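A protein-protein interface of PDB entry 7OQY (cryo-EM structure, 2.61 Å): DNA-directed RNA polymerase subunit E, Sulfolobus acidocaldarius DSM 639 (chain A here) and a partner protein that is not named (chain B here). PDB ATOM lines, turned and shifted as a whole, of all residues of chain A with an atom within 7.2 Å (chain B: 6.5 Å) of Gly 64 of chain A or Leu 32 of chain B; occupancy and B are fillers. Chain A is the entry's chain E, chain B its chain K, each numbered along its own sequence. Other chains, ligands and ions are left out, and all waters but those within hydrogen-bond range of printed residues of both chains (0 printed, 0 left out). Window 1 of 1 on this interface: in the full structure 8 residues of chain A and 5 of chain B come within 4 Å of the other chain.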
ATOM      1  N   ARG A  12      10.273  36.287 -15.799  1.00  0.00           N
ATOM      2  CA  ARG A  12       9.963  35.045 -16.495  1.00  0.00           C
ATOM      3  C   ARG A  12      10.150  35.242 -17.995  1.00  0.00           C
ATOM      4  O   ARG A  12       9.533  36.131 -18.589  1.00  0.00           O
ATOM      5  CB  ARG A  12       8.537  34.595 -16.179  1.00  0.00           C
ATOM      6  CG  ARG A  12       7.976  33.565 -17.139  1.00  0.00           C
ATOM      7  CD  ARG A  12       6.538  33.220 -16.796  1.00  0.00           C
ATOM      8  NE  ARG A  12       6.039  32.092 -17.573  1.00  0.00           N
ATOM      9  CZ  ARG A  12       5.567  32.181 -18.809  1.00  0.00           C
ATOM     10  NH1 ARG A  12       5.514  33.338 -19.447  1.00  0.00           N
ATOM     11  NH2 ARG A  12       5.141  31.080 -19.422  1.00  0.00           N
ATOM     12  N   ILE A  13      10.992  34.408 -18.599  1.00  0.00           N
ATOM     13  CA  ILE A  13      11.306  34.490 -20.023  1.00  0.00           C
ATOM     14  C   ILE A  13      10.495  33.412 -20.741  1.00  0.00           C
ATOM     15  O   ILE A  13      10.779  32.218 -20.559  1.00  0.00           O
ATOM     16  CB  ILE A  13      12.808  34.313 -20.279  1.00  0.00           C
ATOM     17  CG1 ILE A  13      13.609  35.372 -19.518  1.00  0.00           C
ATOM     18  CG2 ILE A  13      13.105  34.359 -21.769  1.00  0.00           C
ATOM     19  CD1 ILE A  13      13.664  36.715 -20.204  1.00  0.00           C
ATOM     20  N   PRO A  14       9.502  33.775 -21.557  1.00  0.00           N
ATOM     21  CA  PRO A  14       8.696  32.754 -22.223  1.00  0.00           C
ATOM     22  C   PRO A  14       9.525  31.970 -23.223  1.00  0.00           C
ATOM     23  O   PRO A  14      10.515  32.485 -23.771  1.00  0.00           O
ATOM     24  CB  PRO A  14       7.598  33.574 -22.925  1.00  0.00           C
ATOM     25  CG  PRO A  14       7.599  34.898 -22.235  1.00  0.00           C
ATOM     26  CD  PRO A  14       9.015  35.135 -21.835  1.00  0.00           C
ATOM     27  N   PRO A  15       9.165  30.711 -23.488  1.00  0.00           N
ATOM     28  CA  PRO A  15       9.953  29.901 -24.433  1.00  0.00           C
ATOM     29  C   PRO A  15      10.003  30.464 -25.841  1.00  0.00           C
ATOM     30  O   PRO A  15      10.944  30.151 -26.580  1.00  0.00           O
ATOM     31  CB  PRO A  15       9.245  28.540 -24.404  1.00  0.00           C
ATOM     32  CG  PRO A  15       8.537  28.509 -23.097  1.00  0.00           C
ATOM     33  CD  PRO A  15       8.114  29.921 -22.826  1.00  0.00           C
ATOM     34  N   PHE A  18      13.314  32.516 -26.622  1.00  0.00           N
ATOM     35  CA  PHE A  18      14.615  31.902 -26.409  1.00  0.00           C
ATOM     36  C   PHE A  18      15.544  32.216 -27.580  1.00  0.00           C
ATOM     37  O   PHE A  18      15.126  32.703 -28.634  1.00  0.00           O
ATOM     38  CB  PHE A  18      14.477  30.389 -26.240  1.00  0.00           C
ATOM     39  CG  PHE A  18      13.982  29.965 -24.884  1.00  0.00           C
ATOM     40  CD1 PHE A  18      13.644  30.902 -23.924  1.00  0.00           C
ATOM     41  CD2 PHE A  18      13.851  28.621 -24.573  1.00  0.00           C
ATOM     42  CE1 PHE A  18      13.188  30.508 -22.683  1.00  0.00           C
ATOM     43  CE2 PHE A  18      13.395  28.223 -23.334  1.00  0.00           C
ATOM     44  CZ  PHE A  18      13.063  29.168 -22.388  1.00  0.00           C
ATOM     45  N   ILE A  59      13.896  26.236 -13.748  1.00  0.00           N
ATOM     46  CA  ILE A  59      12.671  25.728 -14.352  1.00  0.00           C
ATOM     47  C   ILE A  59      11.813  25.107 -13.260  1.00  0.00           C
ATOM     48  O   ILE A  59      12.323  24.409 -12.376  1.00  0.00           O
ATOM     49  CB  ILE A  59      12.980  24.704 -15.460  1.00  0.00           C
ATOM     50  CG1 ILE A  59      14.018  25.272 -16.428  1.00  0.00           C
ATOM     51  CG2 ILE A  59      11.715  24.327 -16.206  1.00  0.00           C
ATOM     52  CD1 ILE A  59      14.721  24.223 -17.249  1.00  0.00           C
ATOM     53  N   ILE A  60      10.509  25.370 -13.316  1.00  0.00           N
ATOM     54  CA  ILE A  60       9.563  24.869 -12.331  1.00  0.00           C
ATOM     55  C   ILE A  60       8.621  23.878 -13.008  1.00  0.00           C
ATOM     56  O   ILE A  60       8.611  23.724 -14.229  1.00  0.00           O
ATOM     57  CB  ILE A  60       8.769  26.004 -11.655  1.00  0.00           C
ATOM     58  CG1 ILE A  60       7.818  26.661 -12.654  1.00  0.00           C
ATOM     59  CG2 ILE A  60       9.715  27.033 -11.066  1.00  0.00           C
ATOM     60  CD1 ILE A  60       6.816  27.590 -12.015  1.00  0.00           C
ATOM     61  N   PHE A  61       7.829  23.195 -12.186  1.00  0.00           N
ATOM     62  CA  PHE A  61       6.868  22.229 -12.700  1.00  0.00           C
ATOM     63  C   PHE A  61       5.715  22.935 -13.401  1.00  0.00           C
ATOM     64  O   PHE A  61       5.195  23.943 -12.916  1.00  0.00           O
ATOM     65  CB  PHE A  61       6.326  21.360 -11.565  1.00  0.00           C
ATOM     66  CG  PHE A  61       7.090  20.088 -11.352  1.00  0.00           C
ATOM     67  CD1 PHE A  61       7.359  19.239 -12.410  1.00  0.00           C
ATOM     68  CD2 PHE A  61       7.524  19.732 -10.087  1.00  0.00           C
ATOM     69  CE1 PHE A  61       8.057  18.065 -12.212  1.00  0.00           C
ATOM     70  CE2 PHE A  61       8.220  18.558  -9.885  1.00  0.00           C
ATOM     71  CZ  PHE A  61       8.486  17.725 -10.948  1.00  0.00           C
ATOM     72  N   GLY A  62       5.313  22.394 -14.549  1.00  0.00           N
ATOM     73  CA  GLY A  62       4.155  22.890 -15.261  1.00  0.00           C
ATOM     74  C   GLY A  62       4.391  24.102 -16.133  1.00  0.00           C
ATOM     75  O   GLY A  62       3.439  24.589 -16.754  1.00  0.00           O
ATOM     76  N   ASP A  63       5.619  24.607 -16.203  1.00  0.00           N
ATOM     77  CA  ASP A  63       5.943  25.770 -17.014  1.00  0.00           C
ATOM     78  C   ASP A  63       7.166  25.467 -17.865  1.00  0.00           C
ATOM     79  O   ASP A  63       8.073  24.754 -17.429  1.00  0.00           O
ATOM     80  CB  ASP A  63       6.205  27.000 -16.138  1.00  0.00           C
ATOM     81  CG  ASP A  63       5.772  28.291 -16.802  1.00  0.00           C
ATOM     82  OD1 ASP A  63       5.339  28.245 -17.971  1.00  0.00           O
ATOM     83  OD2 ASP A  63       5.864  29.352 -16.153  1.00  0.00           O
ATOM     84  N   GLY A  64       7.183  26.009 -19.078  1.00  0.00           N
ATOM     85  CA  GLY A  64       8.319  25.842 -19.961  1.00  0.00           C
ATOM     86  C   GLY A  64       9.282  27.007 -19.890  1.00  0.00           C
ATOM     87  O   GLY A  64      10.399  26.937 -20.409  1.00  0.00           O
ATOM     88  N   ALA A  65       8.856  28.085 -19.241  1.00  0.00           N
ATOM     89  CA  ALA A  65       9.643  29.302 -19.159  1.00  0.00           C
ATOM     90  C   ALA A  65      10.739  29.180 -18.105  1.00  0.00           C
ATOM     91  O   ALA A  65      10.677  28.350 -17.194  1.00  0.00           O
ATOM     92  CB  ALA A  65       8.745  30.495 -18.838  1.00  0.00           C
ATOM     93  N   THR A  66      11.755  30.027 -18.243  1.00  0.00           N
ATOM     94  CA  THR A  66      12.834  30.142 -17.276  1.00  0.00           C
ATOM     95  C   THR A  66      12.669  31.427 -16.476  1.00  0.00           C
ATOM     96  O   THR A  66      12.171  32.433 -16.983  1.00  0.00           O
ATOM     97  CB  THR A  66      14.205  30.131 -17.958  1.00  0.00           C
ATOM     98  OG1 THR A  66      14.243  31.136 -18.976  1.00  0.00           O
ATOM     99  CG2 THR A  66      14.483  28.775 -18.584  1.00  0.00           C
ATOM    100  N   TYR A  67      13.089  31.382 -15.214  1.00  0.00           N
ATOM    101  CA  TYR A  67      12.954  32.504 -14.294  1.00  0.00           C
ATOM    102  C   TYR A  67      14.342  32.990 -13.904  1.00  0.00           C
ATOM    103  O   TYR A  67      15.145  32.217 -13.373  1.00  0.00           O
ATOM    104  CB  TYR A  67      12.152  32.101 -13.055  1.00  0.00           C
ATOM    105  CG  TYR A  67      10.697  31.790 -13.330  1.00  0.00           C
ATOM    106  CD1 TYR A  67      10.327  30.625 -13.991  1.00  0.00           C
ATOM    107  CD2 TYR A  67       9.693  32.655 -12.925  1.00  0.00           C
ATOM    108  CE1 TYR A  67       9.002  30.336 -14.243  1.00  0.00           C
ATOM    109  CE2 TYR A  67       8.365  32.375 -13.172  1.00  0.00           C
ATOM    110  CZ  TYR A  67       8.025  31.213 -13.832  1.00  0.00           C
ATOM    111  OH  TYR A  67       6.704  30.929 -14.081  1.00  0.00           O
ATOM    112  N   ILE B  27      13.762  15.544 -20.042  1.00  0.00           N
ATOM    113  CA  ILE B  27      13.020  15.306 -21.275  1.00  0.00           C
ATOM    114  C   ILE B  27      11.640  15.945 -21.202  1.00  0.00           C
ATOM    115  O   ILE B  27      11.181  16.568 -22.167  1.00  0.00           O
ATOM    116  CB  ILE B  27      12.944  13.797 -21.571  1.00  0.00           C
ATOM    117  CG1 ILE B  27      14.235  13.331 -22.243  1.00  0.00           C
ATOM    118  CG2 ILE B  27      11.756  13.478 -22.462  1.00  0.00           C
ATOM    119  CD1 ILE B  27      14.360  11.833 -22.352  1.00  0.00           C
ATOM    120  N   SER B  28      10.960  15.821 -20.058  1.00  0.00           N
ATOM    121  CA  SER B  28       9.633  16.412 -19.931  1.00  0.00           C
ATOM    122  C   SER B  28       9.687  17.933 -20.019  1.00  0.00           C
ATOM    123  O   SER B  28       8.855  18.549 -20.696  1.00  0.00           O
ATOM    124  CB  SER B  28       8.983  15.971 -18.621  1.00  0.00           C
ATOM    125  OG  SER B  28       9.680  16.489 -17.504  1.00  0.00           O
ATOM    126  N   ALA B  29      10.658  18.559 -19.344  1.00  0.00           N
ATOM    127  CA  ALA B  29      10.774  20.013 -19.407  1.00  0.00           C
ATOM    128  C   ALA B  29      11.091  20.484 -20.821  1.00  0.00           C
ATOM    129  O   ALA B  29      10.503  21.460 -21.308  1.00  0.00           O
ATOM    130  CB  ALA B  29      11.842  20.499 -18.430  1.00  0.00           C
ATOM    131  N   ARG B  30      12.018  19.801 -21.497  1.00  0.00           N
ATOM    132  CA  ARG B  30      12.370  20.182 -22.858  1.00  0.00           C
ATOM    133  C   ARG B  30      11.183  20.035 -23.797  1.00  0.00           C
ATOM    134  O   ARG B  30      10.941  20.905 -24.637  1.00  0.00           O
ATOM    135  CB  ARG B  30      13.551  19.349 -23.349  1.00  0.00           C
ATOM    136  CG  ARG B  30      14.073  19.766 -24.709  1.00  0.00           C
ATOM    137  CD  ARG B  30      14.295  21.263 -24.776  1.00  0.00           C
ATOM    138  NE  ARG B  30      14.742  21.687 -26.096  1.00  0.00           N
ATOM    139  CZ  ARG B  30      14.756  22.946 -26.512  1.00  0.00           C
ATOM    140  NH1 ARG B  30      14.351  23.934 -25.735  1.00  0.00           N
ATOM    141  NH2 ARG B  30      15.185  23.217 -27.741  1.00  0.00           N
ATOM    142  N   ALA B  31      10.423  18.945 -23.668  1.00  0.00           N
ATOM    143  CA  ALA B  31       9.251  18.760 -24.519  1.00  0.00           C
ATOM    144  C   ALA B  31       8.196  19.824 -24.249  1.00  0.00           C
ATOM    145  O   ALA B  31       7.588  20.361 -25.184  1.00  0.00           O
ATOM    146  CB  ALA B  31       8.670  17.363 -24.315  1.00  0.00           C
ATOM    147  N   LEU B  32       7.967  20.149 -22.973  1.00  0.00           N
ATOM    148  CA  LEU B  32       6.972  21.161 -22.640  1.00  0.00           C
ATOM    149  C   LEU B  32       7.349  22.520 -23.210  1.00  0.00           C
ATOM    150  O   LEU B  32       6.500  23.224 -23.765  1.00  0.00           O
ATOM    151  CB  LEU B  32       6.792  21.251 -21.126  1.00  0.00           C
ATOM    152  CG  LEU B  32       5.857  22.360 -20.642  1.00  0.00           C
ATOM    153  CD1 LEU B  32       4.481  22.218 -21.268  1.00  0.00           C
ATOM    154  CD2 LEU B  32       5.760  22.360 -19.131  1.00  0.00           C
ATOM    155  N   GLN B  33       8.621  22.907 -23.096  1.00  0.00           N
ATOM    156  CA  GLN B  33       9.007  24.210 -23.625  1.00  0.00           C
ATOM    157  C   GLN B  33       9.231  24.192 -25.130  1.00  0.00           C
ATOM    158  O   GLN B  33       9.271  25.261 -25.747  1.00  0.00           O
ATOM    159  CB  GLN B  33      10.264  24.726 -22.920  1.00  0.00           C
ATOM    160  CG  GLN B  33      11.514  23.919 -23.168  1.00  0.00           C
ATOM    161  CD  GLN B  33      12.682  24.409 -22.339  1.00  0.00           C
ATOM    162  OE1 GLN B  33      12.563  25.381 -21.597  1.00  0.00           O
ATOM    163  NE2 GLN B  33      13.818  23.739 -22.462  1.00  0.00           N
ATOM    164  N   LEU B  34       9.362  23.013 -25.735  1.00  0.00           N
ATOM    165  CA  LEU B  34       9.472  22.907 -27.182  1.00  0.00           C
ATOM    166  C   LEU B  34       8.107  22.957 -27.853  1.00  0.00           C
ATOM    167  O   LEU B  34       7.994  23.437 -28.986  1.00  0.00           O
ATOM    168  CB  LEU B  34      10.210  21.616 -27.535  1.00  0.00           C
ATOM    169  CG  LEU B  34      10.538  21.256 -28.979  1.00  0.00           C
ATOM    170  CD1 LEU B  34      11.472  22.288 -29.578  1.00  0.00           C
ATOM    171  CD2 LEU B  34      11.173  19.881 -29.016  1.00  0.00           C
ATOM    172  N   SER B  35       7.066  22.467 -27.176  1.00  0.00           N
ATOM    173  CA  SER B  35       5.706  22.606 -27.678  1.00  0.00           C
ATOM    174  C   SER B  35       5.156  24.016 -27.516  1.00  0.00           C
ATOM    175  O   SER B  35       4.121  24.332 -28.112  1.00  0.00           O
ATOM    176  CB  SER B  35       4.780  21.612 -26.975  1.00  0.00           C
ATOM    177  OG  SER B  35       4.416  22.076 -25.688  1.00  0.00           O
ATOM    178  N   MET B  36       5.815  24.864 -26.731  1.00  0.00           N
ATOM    179  CA  MET B  36       5.367  26.228 -26.484  1.00  0.00           C
ATOM    180  C   MET B  36       5.946  27.236 -27.467  1.00  0.00           C
ATOM    181  O   MET B  36       5.681  28.434 -27.328  1.00  0.00           O
ATOM    182  CB  MET B  36       5.723  26.648 -25.057  1.00  0.00           C
ATOM    183  CG  MET B  36       4.775  26.127 -23.994  1.00  0.00           C
ATOM    184  SD  MET B  36       4.816  27.144 -22.505  1.00  0.00           S
ATOM    185  CE  MET B  36       3.965  26.085 -21.341  1.00  0.00           C
ATOM    186  N   GLY B  37       6.732  26.793 -28.443  1.00  0.00           N
ATOM    187  CA  GLY B  37       7.257  27.678 -29.467  1.00  0.00           C
ATOM    188  C   GLY B  37       8.766  27.758 -29.551  1.00  0.00           C
ATOM    189  O   GLY B  37       9.276  28.554 -30.352  1.00  0.00           O
ATOM    190  N   VAL B  52       7.102  16.318 -30.092  1.00  0.00           N
ATOM    191  CA  VAL B  52       8.027  17.075 -29.254  1.00  0.00           C
ATOM    192  C   VAL B  52       8.874  16.147 -28.392  1.00  0.00           C
ATOM    193  O   VAL B  52      10.053  16.422 -28.139  1.00  0.00           O
ATOM    194  CB  VAL B  52       7.262  18.102 -28.400  1.00  0.00           C
ATOM    195  CG1 VAL B  52       6.808  19.269 -29.258  1.00  0.00           C
ATOM    196  CG2 VAL B  52       6.074  17.452 -27.710  1.00  0.00           C
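Of the 12 printed residues of chain B, 3 touch a printed residue of chain A.
Hydrophobic or aromatic side chains of chain A that line the printed part of chain B: Pro 15 and Phe 18.
Among the printed residues, no Asp or Glu carboxylate lies within 4 Å of a Lys or Arg side-chain nitrogen of the other chain.
Gly 64 of chain A touches just these residues of chain B: Leu 32, Gln 33 and Met 36.
Leu 32 of chain B touches just these residues of chain A: Gly 62, Asp 63 and Gly 64.
Printed residues of chain B within 4 Å of Asp 63 of chain A: Leu 32 (3.6 Å).
Of the printed residues of chain A, Gln 33 of chain B touches Pro 15 (3.5 Å), Phe 18 (3.4 Å) and Gly 64 (2.9 Å).
Printed residues of chain B within 4 Å of Pro 15 of chain A: Gln 33 (3.5 Å) and Met 36 (3.9 Å).
The nearest printed residue of chain A that does not touch Gln 33 of chain B is Thr 66 of chain A (4.9 Å).
O of Gly 64 of chain A lies close to OE1 of Gln 33 of chain B, 2.9 Å away.
OD2 of Asp 63 of chain A lies within salt-bridge range of NE of Arg 12 of chain A.
The side-chain hydroxyl (OH) of Tyr 67 of chain A lies within hydrogen-bond range of the side-chain carboxylate (OD2) of Asp 63 of chain A (2.7 Å).
The side-chain amide nitrogen of Gln 33 of chain B lies close to the guanidinium group of Arg 30 of chain B.
The side-chain hydroxyl (OG) of Ser 35 of chain B sits at hydrogen-bond distance from the backbone carbonyl oxygen (O) of Leu 32 of chain B (3.1 Å).
CB of Pro 15 of chain A touches O of Gln 33 of chain B (3.5 Å).
CG of Pro 15 of chain A touches CB of Met 36 of chain B, 3.9 Å away.
OE1 of Gln 33 of chain B touches CE2 of Phe 18 of chain A, at 3.4 Å.
CD2 of Leu 32 of chain B touches C of Gly 62 of chain A (3.7 Å).
CD2 of Leu 32 of chain B touches C of Asp 63 of chain A, at 3.6 Å.
Leu 32 of chain B touches Gly 64 of chain A.
Gly 64 of chain A touches Met 36 of chain B.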
